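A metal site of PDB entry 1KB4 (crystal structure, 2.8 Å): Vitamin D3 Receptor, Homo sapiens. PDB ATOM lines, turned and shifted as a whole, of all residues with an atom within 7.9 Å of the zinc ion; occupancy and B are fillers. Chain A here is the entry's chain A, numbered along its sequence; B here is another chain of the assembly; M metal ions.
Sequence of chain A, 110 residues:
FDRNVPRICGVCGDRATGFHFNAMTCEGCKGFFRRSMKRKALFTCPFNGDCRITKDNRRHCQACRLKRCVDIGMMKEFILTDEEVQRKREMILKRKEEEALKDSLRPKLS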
ATOM      1  N   ILE A   8      -6.524  10.100   4.990  1.00  0.00           N
ATOM      2  CA  ILE A   8      -7.176  11.156   4.250  1.00  0.00           C
ATOM      3  C   ILE A   8      -8.174  11.896   5.151  1.00  0.00           C
ATOM      4  O   ILE A   8      -8.834  11.299   5.974  1.00  0.00           O
ATOM      5  CB  ILE A   8      -7.943  10.584   3.032  1.00  0.00           C
ATOM      6  CG1 ILE A   8      -7.043   9.585   2.296  1.00  0.00           C
ATOM      7  CG2 ILE A   8      -8.335  11.702   2.098  1.00  0.00           C
ATOM      8  CD1 ILE A   8      -7.365   9.388   0.785  1.00  0.00           C
ATOM      9  N   CYS A   9      -8.284  13.203   4.975  1.00  0.00           N
ATOM     10  CA  CYS A   9      -9.239  13.931   5.778  1.00  0.00           C
ATOM     11  C   CYS A   9     -10.622  13.429   5.436  1.00  0.00           C
ATOM     12  O   CYS A   9     -11.013  13.475   4.264  1.00  0.00           O
ATOM     13  CB  CYS A   9      -9.224  15.411   5.447  1.00  0.00           C
ATOM     14  SG  CYS A   9     -10.206  16.349   6.590  1.00  0.00           S
ATOM     15  N   GLY A  10     -11.364  12.984   6.454  1.00  0.00           N
ATOM     16  CA  GLY A  10     -12.713  12.510   6.263  1.00  0.00           C
ATOM     17  C   GLY A  10     -13.692  13.648   6.001  1.00  0.00           C
ATOM     18  O   GLY A  10     -14.873  13.437   5.851  1.00  0.00           O
ATOM     19  N   VAL A  11     -13.213  14.875   5.939  1.00  0.00           N
ATOM     20  CA  VAL A  11     -14.121  15.967   5.699  1.00  0.00           C
ATOM     21  C   VAL A  11     -13.927  16.546   4.306  1.00  0.00           C
ATOM     22  O   VAL A  11     -14.889  16.727   3.574  1.00  0.00           O
ATOM     23  CB  VAL A  11     -13.954  17.060   6.799  1.00  0.00           C
ATOM     24  CG1 VAL A  11     -14.813  18.202   6.566  1.00  0.00           C
ATOM     25  CG2 VAL A  11     -14.273  16.486   8.144  1.00  0.00           C
ATOM     26  N   CYS A  12     -12.695  16.787   3.911  1.00  0.00           N
ATOM     27  CA  CYS A  12     -12.421  17.400   2.633  1.00  0.00           C
ATOM     28  C   CYS A  12     -11.540  16.602   1.679  1.00  0.00           C
ATOM     29  O   CYS A  12     -11.248  17.028   0.563  1.00  0.00           O
ATOM     30  CB  CYS A  12     -11.815  18.763   2.861  1.00  0.00           C
ATOM     31  SG  CYS A  12     -10.227  18.635   3.657  1.00  0.00           S
ATOM     32  N   GLY A  13     -11.087  15.438   2.119  1.00  0.00           N
ATOM     33  CA  GLY A  13     -10.250  14.643   1.232  1.00  0.00           C
ATOM     34  C   GLY A  13      -8.775  14.992   1.224  1.00  0.00           C
ATOM     35  O   GLY A  13      -7.941  14.263   0.678  1.00  0.00           O
ATOM     36  N   ASP A  14      -8.442  16.117   1.845  1.00  0.00           N
ATOM     37  CA  ASP A  14      -7.071  16.538   1.928  1.00  0.00           C
ATOM     38  C   ASP A  14      -6.207  15.556   2.764  1.00  0.00           C
ATOM     39  O   ASP A  14      -6.738  14.696   3.482  1.00  0.00           O
ATOM     40  CB  ASP A  14      -7.036  17.932   2.520  1.00  0.00           C
ATOM     41  CG  ASP A  14      -5.708  18.552   2.360  1.00  0.00           C
ATOM     42  OD1 ASP A  14      -5.560  19.755   2.665  1.00  0.00           O
ATOM     43  OD2 ASP A  14      -4.803  17.811   1.922  1.00  0.00           O
ATOM     44  N   ARG A  15      -4.876  15.683   2.667  1.00  0.00           N
ATOM     45  CA  ARG A  15      -3.985  14.770   3.400  1.00  0.00           C
ATOM     46  C   ARG A  15      -4.234  14.958   4.881  1.00  0.00           C
ATOM     47  O   ARG A  15      -4.248  16.095   5.388  1.00  0.00           O
ATOM     48  CB  ARG A  15      -2.490  15.041   3.061  1.00  0.00           C
ATOM     49  N   ALA A  16      -4.444  13.874   5.586  1.00  0.00           N
ATOM     50  CA  ALA A  16      -4.680  14.021   7.000  1.00  0.00           C
ATOM     51  C   ALA A  16      -3.393  13.909   7.790  1.00  0.00           C
ATOM     52  O   ALA A  16      -2.428  13.335   7.318  1.00  0.00           O
ATOM     53  CB  ALA A  16      -5.675  12.970   7.454  1.00  0.00           C
ATOM     54  N   MET A  24     -10.131  11.140  11.752  1.00  0.00           N
ATOM     55  CA  MET A  24      -8.983  11.324  10.861  1.00  0.00           C
ATOM     56  C   MET A  24      -9.193  12.603  10.072  1.00  0.00           C
ATOM     57  O   MET A  24     -10.059  12.667   9.243  1.00  0.00           O
ATOM     58  CB  MET A  24      -8.867  10.138   9.924  1.00  0.00           C
ATOM     59  CG  MET A  24      -7.705  10.191   9.000  1.00  0.00           C
ATOM     60  SD  MET A  24      -6.008  10.360   9.715  1.00  0.00           S
ATOM     61  CE  MET A  24      -5.861   8.782  10.757  1.00  0.00           C
ATOM     62  N   THR A  25      -8.398  13.632  10.317  1.00  0.00           N
ATOM     63  CA  THR A  25      -8.632  14.888   9.603  1.00  0.00           C
ATOM     64  C   THR A  25      -7.360  15.654   9.222  1.00  0.00           C
ATOM     65  O   THR A  25      -6.271  15.370   9.731  1.00  0.00           O
ATOM     66  CB  THR A  25      -9.517  15.825  10.464  1.00  0.00           C
ATOM     67  OG1 THR A  25      -8.921  15.991  11.749  1.00  0.00           O
ATOM     68  CG2 THR A  25     -10.880  15.243  10.681  1.00  0.00           C
ATOM     69  N   CYS A  26      -7.522  16.630   8.337  1.00  0.00           N
ATOM     70  CA  CYS A  26      -6.419  17.470   7.885  1.00  0.00           C
ATOM     71  C   CYS A  26      -6.274  18.598   8.901  1.00  0.00           C
ATOM     72  O   CYS A  26      -7.154  18.813   9.713  1.00  0.00           O
ATOM     73  CB  CYS A  26      -6.724  18.030   6.498  1.00  0.00           C
ATOM     74  SG  CYS A  26      -7.974  19.335   6.397  1.00  0.00           S
ATOM     75  N   GLU A  27      -5.163  19.333   8.868  1.00  0.00           N
ATOM     76  CA  GLU A  27      -4.935  20.432   9.811  1.00  0.00           C
ATOM     77  C   GLU A  27      -5.904  21.570   9.693  1.00  0.00           C
ATOM     78  O   GLU A  27      -6.147  22.262  10.674  1.00  0.00           O
ATOM     79  CB  GLU A  27      -3.534  20.999   9.679  1.00  0.00           C
ATOM     80  CG  GLU A  27      -2.432  20.123  10.268  1.00  0.00           C
ATOM     81  CD  GLU A  27      -2.602  19.889  11.758  1.00  0.00           C
ATOM     82  OE1 GLU A  27      -2.881  20.883  12.475  1.00  0.00           O
ATOM     83  OE2 GLU A  27      -2.426  18.729  12.201  1.00  0.00           O
ATOM     84  N   GLY A  28      -6.430  21.797   8.490  1.00  0.00           N
ATOM     85  CA  GLY A  28      -7.396  22.856   8.292  1.00  0.00           C
ATOM     86  C   GLY A  28      -8.711  22.542   8.983  1.00  0.00           C
ATOM     87  O   GLY A  28      -9.260  23.381   9.690  1.00  0.00           O
ATOM     88  N   CYS A  29      -9.210  21.313   8.829  1.00  0.00           N
ATOM     89  CA  CYS A  29     -10.479  20.942   9.428  1.00  0.00           C
ATOM     90  C   CYS A  29     -10.433  20.765  10.930  1.00  0.00           C
ATOM     91  O   CYS A  29     -11.452  20.820  11.611  1.00  0.00           O
ATOM     92  CB  CYS A  29     -11.045  19.712   8.718  1.00  0.00           C
ATOM     93  SG  CYS A  29     -11.526  20.082   6.954  1.00  0.00           S
ATOM     94  N   LYS A  30      -9.247  20.559  11.476  1.00  0.00           N
ATOM     95  CA  LYS A  30      -9.115  20.444  12.906  1.00  0.00           C
ATOM     96  C   LYS A  30      -9.304  21.892  13.448  1.00  0.00           C
ATOM     97  O   LYS A  30     -10.089  22.155  14.367  1.00  0.00           O
ATOM     98  CB  LYS A  30      -7.706  19.893  13.227  1.00  0.00           C
ATOM     99  CG  LYS A  30      -6.875  20.614  14.326  1.00  0.00           C
ATOM    100  CD  LYS A  30      -5.522  19.953  14.464  1.00  0.00           C
ATOM    101  CE  LYS A  30      -4.523  20.800  15.238  1.00  0.00           C
ATOM    102  NZ  LYS A  30      -3.186  20.101  15.256  1.00  0.00           N
ATOM    103  N   PHE A  32     -10.681  24.340  11.957  1.00  0.00           N
ATOM    104  CA  PHE A  32     -12.015  24.833  11.656  1.00  0.00           C
ATOM    105  C   PHE A  32     -12.992  24.338  12.703  1.00  0.00           C
ATOM    106  O   PHE A  32     -13.862  25.060  13.204  1.00  0.00           O
ATOM    107  CB  PHE A  32     -12.465  24.301  10.310  1.00  0.00           C
ATOM    108  CG  PHE A  32     -13.879  24.607  10.008  1.00  0.00           C
ATOM    109  CD1 PHE A  32     -14.234  25.866   9.572  1.00  0.00           C
ATOM    110  CD2 PHE A  32     -14.856  23.644  10.188  1.00  0.00           C
ATOM    111  CE1 PHE A  32     -15.530  26.155   9.324  1.00  0.00           C
ATOM    112  CE2 PHE A  32     -16.153  23.939   9.948  1.00  0.00           C
ATOM    113  CZ  PHE A  32     -16.491  25.179   9.514  1.00  0.00           C
ATOM    114  N   ILE A  53     -17.723  18.802   0.149  1.00  0.00           N
ATOM    115  CA  ILE A  53     -16.535  19.456   0.642  1.00  0.00           C
ATOM    116  C   ILE A  53     -15.354  18.839  -0.040  1.00  0.00           C
ATOM    117  O   ILE A  53     -15.299  17.628  -0.196  1.00  0.00           O
ATOM    118  CB  ILE A  53     -16.397  19.310   2.189  1.00  0.00           C
ATOM    119  CG1 ILE A  53     -17.725  19.589   2.894  1.00  0.00           C
ATOM    120  CG2 ILE A  53     -15.378  20.286   2.711  1.00  0.00           C
ATOM    121  CD1 ILE A  53     -18.350  20.881   2.480  1.00  0.00           C
ATOM    122  N   THR A  54     -14.431  19.676  -0.501  1.00  0.00           N
ATOM    123  CA  THR A  54     -13.208  19.181  -1.142  1.00  0.00           C
ATOM    124  C   THR A  54     -12.099  20.102  -0.699  1.00  0.00           C
ATOM    125  O   THR A  54     -12.340  21.250  -0.357  1.00  0.00           O
ATOM    126  CB  THR A  54     -13.288  19.131  -2.712  1.00  0.00           C
ATOM    127  OG1 THR A  54     -13.395  20.450  -3.280  1.00  0.00           O
ATOM    128  CG2 THR A  54     -14.454  18.286  -3.161  1.00  0.00           C
ATOM    129  N   LYS A  55     -10.887  19.570  -0.679  1.00  0.00           N
ATOM    130  CA  LYS A  55      -9.720  20.353  -0.284  1.00  0.00           C
ATOM    131  C   LYS A  55      -9.766  21.774  -0.796  1.00  0.00           C
ATOM    132  O   LYS A  55      -9.373  22.683  -0.077  1.00  0.00           O
ATOM    133  CB  LYS A  55      -8.441  19.696  -0.802  1.00  0.00           C
ATOM    134  CG  LYS A  55      -7.151  20.359  -0.320  1.00  0.00           C
ATOM    135  CD  LYS A  55      -6.934  21.765  -0.878  1.00  0.00           C
ATOM    136  CE  LYS A  55      -5.662  22.404  -0.345  1.00  0.00           C
ATOM    137  NZ  LYS A  55      -4.485  21.496  -0.572  1.00  0.00           N
ATOM    138  N   ARG A  58     -13.553  23.867   0.572  1.00  0.00           N
ATOM    139  CA  ARG A  58     -13.988  23.730   1.969  1.00  0.00           C
ATOM    140  C   ARG A  58     -14.135  25.085   2.612  1.00  0.00           C
ATOM    141  O   ARG A  58     -14.865  25.283   3.553  1.00  0.00           O
ATOM    142  CB  ARG A  58     -12.997  22.899   2.762  1.00  0.00           C
ATOM    143  CG  ARG A  58     -11.704  23.577   3.005  1.00  0.00           C
ATOM    144  CD  ARG A  58     -10.650  22.603   3.405  1.00  0.00           C
ATOM    145  NE  ARG A  58      -9.340  23.199   3.295  1.00  0.00           N
ATOM    146  CZ  ARG A  58      -8.192  22.525   3.369  1.00  0.00           C
ATOM    147  NH1 ARG A  58      -8.193  21.208   3.557  1.00  0.00           N
ATOM    148  NH2 ARG A  58      -7.043  23.183   3.221  1.00  0.00           N
ATOM    149  N   ARG A  65     -19.302  22.098   5.927  1.00  0.00           N
ATOM    150  CA  ARG A  65     -18.034  21.581   6.456  1.00  0.00           C
ATOM    151  C   ARG A  65     -18.229  21.091   7.886  1.00  0.00           C
ATOM    152  O   ARG A  65     -17.929  19.945   8.183  1.00  0.00           O
ATOM    153  CB  ARG A  65     -16.985  22.662   6.442  1.00  0.00           C
ATOM    154  CG  ARG A  65     -15.557  22.191   6.627  1.00  0.00           C
ATOM    155  CD  ARG A  65     -14.646  23.355   6.573  1.00  0.00           C
ATOM    156  NE  ARG A  65     -13.242  22.982   6.655  1.00  0.00           N
ATOM    157  CZ  ARG A  65     -12.217  23.853   6.611  1.00  0.00           C
ATOM    158  NH1 ARG A  65     -12.446  25.148   6.471  1.00  0.00           N
ATOM    159  NH2 ARG A  65     -10.983  23.417   6.700  1.00  0.00           N
ATOM    160  N   CYS A  69     -18.099  17.564   9.714  1.00  0.00           N
ATOM    161  CA  CYS A  69     -17.204  17.296  10.825  1.00  0.00           C
ATOM    162  C   CYS A  69     -17.886  16.457  11.867  1.00  0.00           C
ATOM    163  O   CYS A  69     -17.335  15.437  12.348  1.00  0.00           O
ATOM    164  CB  CYS A  69     -16.761  18.567  11.500  1.00  0.00           C
ATOM    165  SG  CYS A  69     -15.367  19.341  10.725  1.00  0.00           S
ATOM    166  N   ILE A  72     -18.832  12.828  10.572  1.00  0.00           N
ATOM    167  CA  ILE A  72     -17.832  11.750  10.592  1.00  0.00           C
ATOM    168  C   ILE A  72     -17.441  11.450  12.028  1.00  0.00           C
ATOM    169  O   ILE A  72     -16.692  10.553  12.309  1.00  0.00           O
ATOM    170  CB  ILE A  72     -16.555  12.066   9.778  1.00  0.00           C
ATOM    171  CG1 ILE A  72     -15.785  13.224  10.356  1.00  0.00           C
ATOM    172  CG2 ILE A  72     -16.949  12.477   8.412  1.00  0.00           C
ATOM    173  CD1 ILE A  72     -14.437  13.401   9.746  1.00  0.00           C
ATOM    174  N   MET A  74     -16.449  14.010  14.682  1.00  0.00           N
ATOM    175  CA  MET A  74     -15.564  14.813  15.514  1.00  0.00           C
ATOM    176  C   MET A  74     -16.349  15.227  16.765  1.00  0.00           C
ATOM    177  O   MET A  74     -17.500  15.613  16.702  1.00  0.00           O
ATOM    178  CB  MET A  74     -15.065  16.039  14.770  1.00  0.00           C
ATOM    179  CG  MET A  74     -14.029  15.719  13.713  1.00  0.00           C
ATOM    180  SD  MET A  74     -13.703  17.154  12.722  1.00  0.00           S
ATOM    181  CE  MET A  74     -12.070  17.479  13.257  1.00  0.00           C
ATOM    182  P    DG B  11      -8.711  26.135   5.761  1.00  0.00           P
ATOM    183  OP1  DG B  11      -8.850  25.697   4.350  1.00  0.00           O
ATOM    184  OP2  DG B  11      -9.475  25.465   6.818  1.00  0.00           O
ATOM    185  O5'  DG B  11      -7.172  25.902   6.060  1.00  0.00           O
ATOM    186  C5'  DG B  11      -6.195  26.400   5.166  1.00  0.00           C
ATOM    187  C4'  DG B  11      -4.826  26.236   5.757  1.00  0.00           C
ATOM    188  O4'  DG B  11      -4.713  27.106   6.881  1.00  0.00           O
ATOM    189  C3'  DG B  11      -4.495  24.858   6.294  1.00  0.00           C
ATOM    190  O3'  DG B  11      -3.114  24.680   6.113  1.00  0.00           O
ATOM    191  C2'  DG B  11      -4.689  25.008   7.780  1.00  0.00           C
ATOM    192  C1'  DG B  11      -4.139  26.389   7.956  1.00  0.00           C
ATOM    193  N9   DG B  11      -4.521  27.057   9.171  1.00  0.00           N
ATOM    194  C8   DG B  11      -5.640  26.811   9.901  1.00  0.00           C
ATOM    195  N7   DG B  11      -5.783  27.631  10.899  1.00  0.00           N
ATOM    196  C5   DG B  11      -4.671  28.453  10.844  1.00  0.00           C
ATOM    197  C6   DG B  11      -4.299  29.543  11.670  1.00  0.00           C
ATOM    198  O6   DG B  11      -4.908  30.015  12.641  1.00  0.00           O
ATOM    199  N1   DG B  11      -3.110  30.116  11.244  1.00  0.00           N
ATOM    200  C2   DG B  11      -2.378  29.715  10.174  1.00  0.00           C
ATOM    201  N2   DG B  11      -1.268  30.447   9.914  1.00  0.00           N
ATOM    202  N3   DG B  11      -2.710  28.686   9.394  1.00  0.00           N
ATOM    203  C4   DG B  11      -3.869  28.105   9.791  1.00  0.00           C
HETATM  204 ZN    ZN M   1     -10.207  18.416   5.930  1.00  0.00          ZN
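Within 4 Å of the zinc ion: Cys 9, Cys 12, Cys 26 and Cys 29. The nearest printed residue that does not touch the zinc ion is Val 11 of chain A (4.1 Å).
The side-chain sulfur (SG) of Cys 9 lies close to the backbone NH (N) of Val 11 of chain A, at 3.4 Å. N of Cys 9 is in hydrogen-bond range of O of Asp 14 (2.6 Å). NH1 of Arg 58 sits close to SG of Cys 12 (3.3 Å). The backbone NH (N) of Asp 14 sits close to the side-chain sulfur (SG) of Cys 12 (3.6 Å). O of Cys 12 sits at hydrogen-bond distance from N of Lys 55, 2.9 Å away. SG of Cys 29 lies close to NE of Arg 65 (3.4 Å). The side-chain sulfur of Cys 26 sits close to the guanidinium group of Arg 58 (3.4 Å). The side-chain sulfur (SG) of Cys 26 lies close to the backbone NH (N) of Gly 28, at 3.6 Å.
The zinc ion is bound by the side-chain sulfur of Cys 9 (2.2 Å), the side-chain sulfur of Cys 12 (2.3 Å), the side-chain sulfur of Cys 29 (2.4 Å) and the side-chain sulfur of Cys 26 (2.5 Å). The zinc ion has four donor atoms within binding distance.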
